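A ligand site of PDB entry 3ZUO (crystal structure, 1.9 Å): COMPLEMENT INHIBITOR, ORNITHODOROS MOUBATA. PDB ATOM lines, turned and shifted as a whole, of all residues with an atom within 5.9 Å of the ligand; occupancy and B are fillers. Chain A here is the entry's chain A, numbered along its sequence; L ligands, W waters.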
ATOM      1  N   PHE A  18      -3.168   0.212  22.453  1.00  0.00           N
ATOM      2  CA  PHE A  18      -2.799   1.471  23.099  1.00  0.00           C
ATOM      3  C   PHE A  18      -1.398   1.397  23.740  1.00  0.00           C
ATOM      4  O   PHE A  18      -1.125   2.153  24.670  1.00  0.00           O
ATOM      5  CB  PHE A  18      -3.835   1.836  24.184  1.00  0.00           C
ATOM      6  CG  PHE A  18      -5.303   1.823  23.803  1.00  0.00           C
ATOM      7  CD1 PHE A  18      -5.692   1.988  22.472  1.00  0.00           C
ATOM      8  CD2 PHE A  18      -6.291   1.741  24.773  1.00  0.00           C
ATOM      9  CE1 PHE A  18      -7.043   2.000  22.128  1.00  0.00           C
ATOM     10  CE2 PHE A  18      -7.632   1.769  24.419  1.00  0.00           C
ATOM     11  CZ  PHE A  18      -8.002   1.908  23.102  1.00  0.00           C
ATOM     12  N   GLY A  21      -1.186   1.227  27.596  1.00  0.00           N
ATOM     13  CA  GLY A  21      -1.428   2.474  28.341  1.00  0.00           C
ATOM     14  C   GLY A  21      -0.174   3.307  28.638  1.00  0.00           C
ATOM     15  O   GLY A  21      -0.210   4.093  29.585  1.00  0.00           O
ATOM     16  N   LYS A  22       0.910   3.158  27.848  1.00  0.00           N
ATOM     17  CA  LYS A  22       2.170   3.883  28.054  1.00  0.00           C
ATOM     18  C   LYS A  22       2.449   4.990  27.022  1.00  0.00           C
ATOM     19  O   LYS A  22       3.400   5.743  27.223  1.00  0.00           O
ATOM     20  CB  LYS A  22       3.348   2.904  28.051  1.00  0.00           C
ATOM     21  CG  LYS A  22       3.315   1.877  29.179  1.00  0.00           C
ATOM     22  CD  LYS A  22       4.588   1.017  29.227  1.00  0.00           C
ATOM     23  CE  LYS A  22       4.380  -0.393  28.723  1.00  0.00           C
ATOM     24  NZ  LYS A  22       5.671  -1.051  28.400  1.00  0.00           N
ATOM     25  N   GLU A  23       1.662   5.092  25.939  1.00  0.00           N
ATOM     26  CA  GLU A  23       1.905   6.081  24.879  1.00  0.00           C
ATOM     27  C   GLU A  23       0.688   6.971  24.603  1.00  0.00           C
ATOM     28  O   GLU A  23      -0.443   6.563  24.809  1.00  0.00           O
ATOM     29  CB  GLU A  23       2.303   5.382  23.577  1.00  0.00           C
ATOM     30  CG  GLU A  23       3.523   4.474  23.682  1.00  0.00           C
ATOM     31  CD  GLU A  23       4.820   5.159  24.055  1.00  0.00           C
ATOM     32  OE1 GLU A  23       4.971   6.370  23.772  1.00  0.00           O
ATOM     33  OE2 GLU A  23       5.707   4.474  24.616  1.00  0.00           O
ATOM     34  N   ALA A  24       0.962   8.186  24.081  1.00  0.00           N
ATOM     35  CA  ALA A  24      -0.086   9.144  23.711  1.00  0.00           C
ATOM     36  C   ALA A  24      -0.497   8.879  22.278  1.00  0.00           C
ATOM     37  O   ALA A  24       0.364   8.655  21.421  1.00  0.00           O
ATOM     38  CB  ALA A  24       0.432  10.563  23.847  1.00  0.00           C
ATOM     39  N   TYR A  25      -1.816   8.895  21.991  1.00  0.00           N
ATOM     40  CA  TYR A  25      -2.370   8.682  20.656  1.00  0.00           C
ATOM     41  C   TYR A  25      -3.156   9.912  20.231  1.00  0.00           C
ATOM     42  O   TYR A  25      -3.818  10.521  21.070  1.00  0.00           O
ATOM     43  CB  TYR A  25      -3.287   7.444  20.641  1.00  0.00           C
ATOM     44  CG  TYR A  25      -2.516   6.148  20.582  1.00  0.00           C
ATOM     45  CD1 TYR A  25      -1.912   5.626  21.720  1.00  0.00           C
ATOM     46  CD2 TYR A  25      -2.353   5.471  19.383  1.00  0.00           C
ATOM     47  CE1 TYR A  25      -1.161   4.456  21.667  1.00  0.00           C
ATOM     48  CE2 TYR A  25      -1.615   4.283  19.318  1.00  0.00           C
ATOM     49  CZ  TYR A  25      -1.034   3.771  20.466  1.00  0.00           C
ATOM     50  OH  TYR A  25      -0.303   2.610  20.436  1.00  0.00           O
ATOM     51  N   ARG A  36     -13.480  16.210  17.922  1.00  0.00           N
ATOM     52  CA  ARG A  36     -12.740  17.245  18.654  1.00  0.00           C
ATOM     53  C   ARG A  36     -11.469  17.642  17.912  1.00  0.00           C
ATOM     54  O   ARG A  36     -10.694  16.761  17.533  1.00  0.00           O
ATOM     55  CB  ARG A  36     -12.393  16.739  20.063  1.00  0.00           C
ATOM     56  CG  ARG A  36     -13.574  16.409  20.955  1.00  0.00           C
ATOM     57  CD  ARG A  36     -14.425  17.621  21.256  1.00  0.00           C
ATOM     58  NE  ARG A  36     -15.279  17.413  22.419  1.00  0.00           N
ATOM     59  CZ  ARG A  36     -16.059  18.334  22.961  1.00  0.00           C
ATOM     60  NH1 ARG A  36     -16.106  19.561  22.446  1.00  0.00           N
ATOM     61  NH2 ARG A  36     -16.801  18.055  24.031  1.00  0.00           N
ATOM     62  N   LEU A  39      -7.499  16.418  18.947  1.00  0.00           N
ATOM     63  CA  LEU A  39      -7.706  15.472  20.033  1.00  0.00           C
ATOM     64  C   LEU A  39      -6.521  14.545  20.251  1.00  0.00           C
ATOM     65  O   LEU A  39      -6.030  13.944  19.290  1.00  0.00           O
ATOM     66  CB  LEU A  39      -8.990  14.647  19.810  1.00  0.00           C
ATOM     67  CG  LEU A  39      -9.465  13.777  20.983  1.00  0.00           C
ATOM     68  CD1 LEU A  39      -9.831  14.626  22.195  1.00  0.00           C
ATOM     69  CD2 LEU A  39     -10.654  12.940  20.569  1.00  0.00           C
ATOM     70  N   GLY A  41      -5.202  11.591  23.277  1.00  0.00           N
ATOM     71  CA  GLY A  41      -5.475  10.809  24.473  1.00  0.00           C
ATOM     72  C   GLY A  41      -4.135  10.329  25.014  1.00  0.00           C
ATOM     73  O   GLY A  41      -3.369   9.745  24.264  1.00  0.00           O
ATOM     74  N   GLU A  42      -3.823  10.616  26.304  1.00  0.00           N
ATOM     75  CA  GLU A  42      -2.537  10.227  26.901  1.00  0.00           C
ATOM     76  C   GLU A  42      -2.707   9.654  28.316  1.00  0.00           C
ATOM     77  O   GLU A  42      -3.748   9.866  28.932  1.00  0.00           O
ATOM     78  CB  GLU A  42      -1.579  11.438  26.906  1.00  0.00           C
ATOM     79  CG  GLU A  42      -1.897  12.517  27.926  1.00  0.00           C
ATOM     80  CD  GLU A  42      -1.080  13.783  27.753  1.00  0.00           C
ATOM     81  OE1 GLU A  42      -1.467  14.619  26.907  1.00  0.00           O
ATOM     82  OE2 GLU A  42      -0.065  13.933  28.466  1.00  0.00           O
ATOM     83  N   PRO A  43      -1.668   8.943  28.854  1.00  0.00           N
ATOM     84  CA  PRO A  43      -1.782   8.387  30.209  1.00  0.00           C
ATOM     85  C   PRO A  43      -1.911   9.467  31.290  1.00  0.00           C
ATOM     86  O   PRO A  43      -1.276  10.518  31.188  1.00  0.00           O
ATOM     87  CB  PRO A  43      -0.490   7.564  30.365  1.00  0.00           C
ATOM     88  CG  PRO A  43       0.016   7.353  28.996  1.00  0.00           C
ATOM     89  CD  PRO A  43      -0.391   8.570  28.236  1.00  0.00           C
ATOM     90  N   ALA A  44      -2.732   9.201  32.315  1.00  0.00           N
ATOM     91  CA  ALA A  44      -2.989  10.127  33.418  1.00  0.00           C
ATOM     92  C   ALA A  44      -2.886   9.384  34.770  1.00  0.00           C
ATOM     93  O   ALA A  44      -3.790   9.471  35.600  1.00  0.00           O
ATOM     94  CB  ALA A  44      -4.367  10.746  33.257  1.00  0.00           C
ATOM     95  N   LEU A  52      -8.475   2.287  33.534  1.00  0.00           N
ATOM     96  CA  LEU A  52      -7.356   2.988  32.912  1.00  0.00           C
ATOM     97  C   LEU A  52      -7.724   4.486  32.735  1.00  0.00           C
ATOM     98  O   LEU A  52      -8.576   4.800  31.915  1.00  0.00           O
ATOM     99  CB  LEU A  52      -7.019   2.338  31.553  1.00  0.00           C
ATOM    100  CG  LEU A  52      -5.722   2.796  30.871  1.00  0.00           C
ATOM    101  CD1 LEU A  52      -4.525   2.025  31.396  1.00  0.00           C
ATOM    102  CD2 LEU A  52      -5.800   2.615  29.370  1.00  0.00           C
ATOM    103  N   PRO A  53      -7.123   5.409  33.541  1.00  0.00           N
ATOM    104  CA  PRO A  53      -7.445   6.830  33.411  1.00  0.00           C
ATOM    105  C   PRO A  53      -6.740   7.441  32.202  1.00  0.00           C
ATOM    106  O   PRO A  53      -5.550   7.186  32.005  1.00  0.00           O
ATOM    107  CB  PRO A  53      -6.957   7.430  34.735  1.00  0.00           C
ATOM    108  CG  PRO A  53      -5.868   6.550  35.169  1.00  0.00           C
ATOM    109  CD  PRO A  53      -6.192   5.173  34.667  1.00  0.00           C
ATOM    110  N   VAL A  54      -7.481   8.218  31.389  1.00  0.00           N
ATOM    111  CA  VAL A  54      -6.946   8.847  30.166  1.00  0.00           C
ATOM    112  C   VAL A  54      -7.258  10.342  30.165  1.00  0.00           C
ATOM    113  O   VAL A  54      -8.394  10.733  30.415  1.00  0.00           O
ATOM    114  CB  VAL A  54      -7.508   8.141  28.905  1.00  0.00           C
ATOM    115  CG1 VAL A  54      -6.975   8.786  27.622  1.00  0.00           C
ATOM    116  CG2 VAL A  54      -7.191   6.657  28.927  1.00  0.00           C
ATOM    117  N   MET A  56      -7.673  13.583  27.940  1.00  0.00           N
ATOM    118  CA  MET A  56      -7.938  14.010  26.571  1.00  0.00           C
ATOM    119  C   MET A  56      -7.691  15.504  26.476  1.00  0.00           C
ATOM    120  O   MET A  56      -8.281  16.251  27.254  1.00  0.00           O
ATOM    121  CB  MET A  56      -9.398  13.725  26.182  1.00  0.00           C
ATOM    122  CG  MET A  56      -9.731  12.255  26.107  1.00  0.00           C
ATOM    123  SD  MET A  56      -9.066  11.490  24.604  1.00  0.00           S
ATOM    124  CE  MET A  56      -9.655   9.856  24.822  1.00  0.00           C
ATOM    125  N   PHE A  58      -7.750  18.838  23.740  1.00  0.00           N
ATOM    126  CA  PHE A  58      -8.300  19.271  22.447  1.00  0.00           C
ATOM    127  C   PHE A  58      -8.562  20.777  22.418  1.00  0.00           C
ATOM    128  O   PHE A  58      -8.370  21.444  23.437  1.00  0.00           O
ATOM    129  CB  PHE A  58      -9.601  18.488  22.163  1.00  0.00           C
ATOM    130  CG  PHE A  58     -10.672  18.660  23.216  1.00  0.00           C
ATOM    131  CD1 PHE A  58     -10.658  17.897  24.374  1.00  0.00           C
ATOM    132  CD2 PHE A  58     -11.700  19.566  23.041  1.00  0.00           C
ATOM    133  CE1 PHE A  58     -11.641  18.060  25.353  1.00  0.00           C
ATOM    134  CE2 PHE A  58     -12.692  19.720  24.008  1.00  0.00           C
ATOM    135  CZ  PHE A  58     -12.650  18.969  25.163  1.00  0.00           C
ATOM    136  N   THR A  67     -10.054  17.140  29.434  1.00  0.00           N
ATOM    137  CA  THR A  67     -11.001  16.373  30.237  1.00  0.00           C
ATOM    138  C   THR A  67     -10.376  15.031  30.661  1.00  0.00           C
ATOM    139  O   THR A  67      -9.454  14.559  29.997  1.00  0.00           O
ATOM    140  CB  THR A  67     -12.314  16.176  29.465  1.00  0.00           C
ATOM    141  OG1 THR A  67     -12.038  15.661  28.159  1.00  0.00           O
ATOM    142  CG2 THR A  67     -13.093  17.476  29.322  1.00  0.00           C
ATOM    143  N   TRP A  69     -11.062  11.121  31.200  1.00  0.00           N
ATOM    144  CA  TRP A  69     -11.931   9.986  30.904  1.00  0.00           C
ATOM    145  C   TRP A  69     -11.381   8.718  31.567  1.00  0.00           C
ATOM    146  O   TRP A  69     -10.175   8.582  31.742  1.00  0.00           O
ATOM    147  CB  TRP A  69     -12.045   9.774  29.386  1.00  0.00           C
ATOM    148  CG  TRP A  69     -12.859  10.826  28.697  1.00  0.00           C
ATOM    149  CD1 TRP A  69     -12.474  12.102  28.423  1.00  0.00           C
ATOM    150  CD2 TRP A  69     -14.182  10.682  28.183  1.00  0.00           C
ATOM    151  NE1 TRP A  69     -13.489  12.773  27.783  1.00  0.00           N
ATOM    152  CE2 TRP A  69     -14.558  11.917  27.617  1.00  0.00           C
ATOM    153  CE3 TRP A  69     -15.113   9.632  28.183  1.00  0.00           C
ATOM    154  CZ2 TRP A  69     -15.809  12.137  27.052  1.00  0.00           C
ATOM    155  CZ3 TRP A  69     -16.353   9.847  27.613  1.00  0.00           C
ATOM    156  CH2 TRP A  69     -16.696  11.082  27.049  1.00  0.00           C
ATOM    157  N   PHE A  71     -11.275   4.659  31.105  1.00  0.00           N
ATOM    158  CA  PHE A  71     -11.461   3.578  30.135  1.00  0.00           C
ATOM    159  C   PHE A  71     -11.591   2.222  30.845  1.00  0.00           C
ATOM    160  O   PHE A  71     -10.803   1.929  31.744  1.00  0.00           O
ATOM    161  CB  PHE A  71     -10.273   3.490  29.161  1.00  0.00           C
ATOM    162  CG  PHE A  71     -10.135   4.477  28.028  1.00  0.00           C
ATOM    163  CD1 PHE A  71     -10.792   5.708  28.069  1.00  0.00           C
ATOM    164  CD2 PHE A  71      -9.298   4.218  26.951  1.00  0.00           C
ATOM    165  CE1 PHE A  71     -10.629   6.633  27.038  1.00  0.00           C
ATOM    166  CE2 PHE A  71      -9.135   5.155  25.928  1.00  0.00           C
ATOM    167  CZ  PHE A  71      -9.800   6.348  25.986  1.00  0.00           C
ATOM    168  N   VAL A  78     -13.861  -1.153  24.115  1.00  0.00           N
ATOM    169  CA  VAL A  78     -13.401  -0.047  24.954  1.00  0.00           C
ATOM    170  C   VAL A  78     -14.583   0.838  25.373  1.00  0.00           C
ATOM    171  O   VAL A  78     -15.188   1.475  24.514  1.00  0.00           O
ATOM    172  CB  VAL A  78     -12.353   0.794  24.183  1.00  0.00           C
ATOM    173  CG1 VAL A  78     -11.775   1.913  25.052  1.00  0.00           C
ATOM    174  CG2 VAL A  78     -11.242  -0.099  23.639  1.00  0.00           C
ATOM    175  N   ALA A  80     -15.567   4.183  27.496  1.00  0.00           N
ATOM    176  CA  ALA A  80     -14.987   5.389  28.071  1.00  0.00           C
ATOM    177  C   ALA A  80     -16.093   6.180  28.783  1.00  0.00           C
ATOM    178  O   ALA A  80     -17.176   6.327  28.224  1.00  0.00           O
ATOM    179  CB  ALA A  80     -14.375   6.236  26.956  1.00  0.00           C
ATOM    180  N   LEU A  82     -17.061   9.830  31.332  1.00  0.00           N
ATOM    181  CA  LEU A  82     -16.739  11.158  31.855  1.00  0.00           C
ATOM    182  C   LEU A  82     -17.959  11.623  32.637  1.00  0.00           C
ATOM    183  O   LEU A  82     -18.944  12.051  32.036  1.00  0.00           O
ATOM    184  CB  LEU A  82     -16.417  12.141  30.717  1.00  0.00           C
ATOM    185  CG  LEU A  82     -16.223  13.619  31.100  1.00  0.00           C
ATOM    186  CD1 LEU A  82     -14.970  13.820  31.903  1.00  0.00           C
ATOM    187  CD2 LEU A  82     -16.173  14.489  29.852  1.00  0.00           C
ATOM    188  N   GLN A  87     -19.343   6.450  26.367  1.00  0.00           N
ATOM    189  CA  GLN A  87     -19.102   6.203  24.949  1.00  0.00           C
ATOM    190  C   GLN A  87     -18.497   4.810  24.807  1.00  0.00           C
ATOM    191  O   GLN A  87     -17.538   4.488  25.515  1.00  0.00           O
ATOM    192  CB  GLN A  87     -18.133   7.242  24.363  1.00  0.00           C
ATOM    193  CG  GLN A  87     -18.671   8.659  24.350  1.00  0.00           C
ATOM    194  CD  GLN A  87     -17.740   9.624  23.646  1.00  0.00           C
ATOM    195  OE1 GLN A  87     -16.705   9.249  23.079  1.00  0.00           O
ATOM    196  NE2 GLN A  87     -18.073  10.905  23.667  1.00  0.00           N
ATOM    197  N   ARG A  89     -16.735   1.876  22.277  1.00  0.00           N
ATOM    198  CA  ARG A  89     -15.939   1.693  21.067  1.00  0.00           C
ATOM    199  C   ARG A  89     -15.467   0.244  20.953  1.00  0.00           C
ATOM    200  O   ARG A  89     -15.420  -0.484  21.939  1.00  0.00           O
ATOM    201  CB  ARG A  89     -14.697   2.610  21.098  1.00  0.00           C
ATOM    202  CG  ARG A  89     -14.960   4.029  20.639  1.00  0.00           C
ATOM    203  CD  ARG A  89     -13.754   4.908  20.897  1.00  0.00           C
ATOM    204  NE  ARG A  89     -13.986   6.301  20.501  1.00  0.00           N
ATOM    205  CZ  ARG A  89     -14.691   7.198  21.187  1.00  0.00           C
ATOM    206  NH1 ARG A  89     -15.270   6.868  22.342  1.00  0.00           N
ATOM    207  NH2 ARG A  89     -14.831   8.434  20.732  1.00  0.00           N
ATOM    208  N   VAL A  91     -12.150  -1.683  18.881  1.00  0.00           N
ATOM    209  CA  VAL A  91     -10.966  -1.532  18.034  1.00  0.00           C
ATOM    210  C   VAL A  91     -11.144  -2.616  16.968  1.00  0.00           C
ATOM    211  O   VAL A  91     -11.044  -3.799  17.273  1.00  0.00           O
ATOM    212  CB  VAL A  91      -9.626  -1.698  18.817  1.00  0.00           C
ATOM    213  CG1 VAL A  91      -8.443  -1.349  17.910  1.00  0.00           C
ATOM    214  CG2 VAL A  91      -9.590  -0.841  20.082  1.00  0.00           C
ATOM    215  N   HIS A 101      -4.498   2.396  14.955  1.00  0.00           N
ATOM    216  CA  HIS A 101      -5.657   1.512  15.014  1.00  0.00           C
ATOM    217  C   HIS A 101      -6.905   2.247  14.577  1.00  0.00           C
ATOM    218  O   HIS A 101      -6.917   3.478  14.536  1.00  0.00           O
ATOM    219  CB  HIS A 101      -5.805   0.908  16.412  1.00  0.00           C
ATOM    220  CG  HIS A 101      -5.934   1.925  17.498  1.00  0.00           C
ATOM    221  ND1 HIS A 101      -4.826   2.403  18.188  1.00  0.00           N
ATOM    222  CD2 HIS A 101      -7.034   2.519  17.986  1.00  0.00           C
ATOM    223  CE1 HIS A 101      -5.302   3.258  19.071  1.00  0.00           C
ATOM    224  NE2 HIS A 101      -6.621   3.360  18.993  1.00  0.00           N
ATOM    225  N   ASP A 103     -11.139   2.514  15.244  1.00  0.00           N
ATOM    226  CA  ASP A 103     -12.239   2.221  16.159  1.00  0.00           C
ATOM    227  C   ASP A 103     -13.563   2.390  15.468  1.00  0.00           C
ATOM    228  O   ASP A 103     -13.706   3.264  14.618  1.00  0.00           O
ATOM    229  CB  ASP A 103     -12.240   3.180  17.351  1.00  0.00           C
ATOM    230  CG  ASP A 103     -11.021   3.134  18.234  1.00  0.00           C
ATOM    231  OD1 ASP A 103     -10.419   2.056  18.343  1.00  0.00           O
ATOM    232  OD2 ASP A 103     -10.705   4.164  18.861  1.00  0.00           O
ATOM    233  N   GLU A 113     -13.119   6.004  13.603  1.00  0.00           N
ATOM    234  CA  GLU A 113     -12.001   6.873  13.971  1.00  0.00           C
ATOM    235  C   GLU A 113     -10.680   6.181  13.733  1.00  0.00           C
ATOM    236  O   GLU A 113     -10.577   4.996  14.029  1.00  0.00           O
ATOM    237  CB  GLU A 113     -12.065   7.201  15.458  1.00  0.00           C
ATOM    238  CG  GLU A 113     -13.231   8.061  15.901  1.00  0.00           C
ATOM    239  CD  GLU A 113     -13.267   8.284  17.403  1.00  0.00           C
ATOM    240  OE1 GLU A 113     -12.684   7.462  18.156  1.00  0.00           O
ATOM    241  OE2 GLU A 113     -13.880   9.282  17.836  1.00  0.00           O
ATOM    242  N   TRP A 115      -6.759   6.375  15.063  1.00  0.00           N
ATOM    243  CA  TRP A 115      -5.874   6.916  16.081  1.00  0.00           C
ATOM    244  C   TRP A 115      -4.478   6.423  15.769  1.00  0.00           C
ATOM    245  O   TRP A 115      -4.328   5.266  15.362  1.00  0.00           O
ATOM    246  CB  TRP A 115      -6.286   6.429  17.459  1.00  0.00           C
ATOM    247  CG  TRP A 115      -7.581   7.000  17.956  1.00  0.00           C
ATOM    248  CD1 TRP A 115      -8.831   6.543  17.689  1.00  0.00           C
ATOM    249  CD2 TRP A 115      -7.733   8.093  18.872  1.00  0.00           C
ATOM    250  NE1 TRP A 115      -9.770   7.301  18.364  1.00  0.00           N
ATOM    251  CE2 TRP A 115      -9.123   8.243  19.106  1.00  0.00           C
ATOM    252  CE3 TRP A 115      -6.838   8.955  19.519  1.00  0.00           C
ATOM    253  CZ2 TRP A 115      -9.622   9.232  19.958  1.00  0.00           C
ATOM    254  CZ3 TRP A 115      -7.341   9.923  20.364  1.00  0.00           C
ATOM    255  CH2 TRP A 115      -8.711  10.064  20.575  1.00  0.00           C
HETATM  256  O1  LIG L   1     -14.217  15.241  26.397  1.00  0.00           O
HETATM  257  C1  LIG L   1     -14.185  15.153  25.146  1.00  0.00           C
HETATM  258  O2  LIG L   1     -15.128  15.473  24.379  1.00  0.00           O
HETATM  259  C2  LIG L   1     -12.900  14.647  24.520  1.00  0.00           C
HETATM  260  C3  LIG L   1     -13.143  13.461  23.575  1.00  0.00           C
HETATM  261  C4  LIG L   1     -13.549  12.215  24.361  1.00  0.00           C
HETATM  262  C5  LIG L   1     -13.628  10.973  23.471  1.00  0.00           C
HETATM  263  O3  LIG L   1     -14.688  11.105  22.528  1.00  0.00           O
HETATM  264  C6  LIG L   1     -13.883   9.745  24.343  1.00  0.00           C
HETATM  265  C7  LIG L   1     -13.211   8.531  24.205  1.00  0.00           C
HETATM  266  C8  LIG L   1     -12.202   8.330  23.267  1.00  0.00           C
HETATM  267  C9  LIG L   1     -11.561   7.101  23.186  1.00  0.00           C
HETATM  268  C10 LIG L   1     -10.511   6.795  22.311  1.00  0.00           C
HETATM  269  C11 LIG L   1      -9.847   5.589  22.223  1.00  0.00           C
HETATM  270  C12 LIG L   1      -8.696   5.446  21.215  1.00  0.00           C
HETATM  271  C13 LIG L   1      -3.473   5.430  28.737  1.00  0.00           C
HETATM  272  O4  LIG L   1      -8.833   4.167  20.575  1.00  0.00           O
HETATM  273  C14 LIG L   1      -3.510   6.379  27.536  1.00  0.00           C
HETATM  274  C15 LIG L   1      -4.545   5.913  26.496  1.00  0.00           C
HETATM  275  C16 LIG L   1      -4.408   6.703  25.203  1.00  0.00           C
HETATM  276  C17 LIG L   1      -5.244   6.120  24.049  1.00  0.00           C
HETATM  277  C18 LIG L   1      -6.078   7.057  23.424  1.00  0.00           C
HETATM  278  C19 LIG L   1      -7.050   6.778  22.452  1.00  0.00           C
HETATM  279  C20 LIG L   1      -7.346   5.506  21.936  1.00  0.00           C
HETATM  280  O   HOH W   1     -13.098  10.982  19.959  1.00  0.00           O
HETATM  281  O   HOH W   2      -1.807   4.525  25.609  1.00  0.00           O
HETATM  282  O   HOH W   3     -16.077  17.118  27.062  1.00  0.00           O
HETATM  283  O   HOH W   4     -16.587  13.013  20.359  1.00  0.00           O
HETATM  284  O   HOH W   5     -16.770  13.778  23.056  1.00  0.00           O
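The side-chain carboxylate (OD2) of Asp 103 lies within hydrogen-bond range of an oxygen (O4) of the ligand (2.5 Å). NH2 of Arg 89 lies within hydrogen-bond range of O3 of the ligand (3.2 Å). The side-chain amide oxygen of Gln 87 is in hydrogen-bond range of an oxygen (O3) of the ligand (2.8 Å). The indole nitrogen of Trp 69 sits at hydrogen-bond distance from an oxygen (O1) of the ligand (2.9 Å). NE2 of His 101 sits at hydrogen-bond distance from O4 of the ligand (2.8 Å). O2 of the ligand lies within salt-bridge range of NE of Arg 36 (2.8 Å). The side-chain hydroxyl of Thr 67 lies within hydrogen-bond range of an oxygen (O1) of the ligand (2.8 Å).
O of Thr 67 sits at hydrogen-bond distance from N of Met 56 (2.9 Å). The side-chain hydroxyl of Thr 67 sits at hydrogen-bond distance from the indole nitrogen of Trp 69, at 3.3 Å. The guanidinium group (NE) of Arg 89 is in salt-bridge range of the side-chain carboxylate (OE1) of Glu 113. O of Trp 115 sits at hydrogen-bond distance from N of His 101. NE1 of Trp 115 sits close to OD2 of Asp 103. The indole nitrogen of Trp 115 lies within hydrogen-bond range of the side-chain carboxylate of Glu 113, at 2.9 Å. The backbone carbonyl oxygen (O) of Leu 52 lies within hydrogen-bond range of the backbone NH (N) of Phe 71. The backbone NH (N) of Asp 103 sits at hydrogen-bond distance from the backbone carbonyl oxygen (O) of Glu 113 (2.8 Å).
CE1 of Phe 18 touches O4 of the ligand, 3.2 Å away. Gly 21 touches the ligand (CA to C13, 3.6 Å). Glu 23 touches the ligand. Tyr 25 touches the ligand (CB to C18, 3.96 Å). Leu 39 touches the ligand. Gly 41 touches the ligand (O to C16, 3.3 Å). Glu 42 touches the ligand (C to C14, 3.5 Å). Pro 43 touches the ligand (N to C14, 3.4 Å). Leu 52 touches the ligand. Val 54 touches the ligand. Met 56 touches the ligand. CE1 of Phe 58 touches C2 of the ligand, at 3.7 Å. Phe 71 touches the ligand. CB of Ala 80 touches C7 of the ligand, 3.8 Å away. Trp 115 touches the ligand (CZ2 to C10, 3.5 Å). Hydrophobic or aromatic side chains within 4 Å of the ligand: Phe 18, Tyr 25, Leu 39, Pro 43, Leu 52, Val 54, Met 56, Phe 58, Trp 69, Phe 71, Ala 80, His 101 and Trp 115. Within 4 Å of the ligand: Phe 18, Gly 21, Glu 23, Tyr 25, Arg 36, Leu 39, Gly 41, Glu 42, Pro 43, Leu 52, Val 54, Met 56, Phe 58, Thr 67, Trp 69, Phe 71, Ala 80, Gln 87, Arg 89, His 101, Asp 103 and Trp 115.
Water W5 bridges an oxygen (O2) of the ligand and the side-chain amide nitrogen of Gln 87. Water W3 bridges an oxygen (O1) of the ligand (2.7 Å) and the guanidinium group (NH2) of Arg 36 (3.3 Å). Water W1 lies within hydrogen-bond range of OE2 of Glu 113, O3 of the ligand and NH2 of Arg 89. Water W2 bridges the backbone carbonyl oxygen of Glu 23 (2.6 Å) and the backbone carbonyl oxygen of Phe 18 (2.6 Å).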
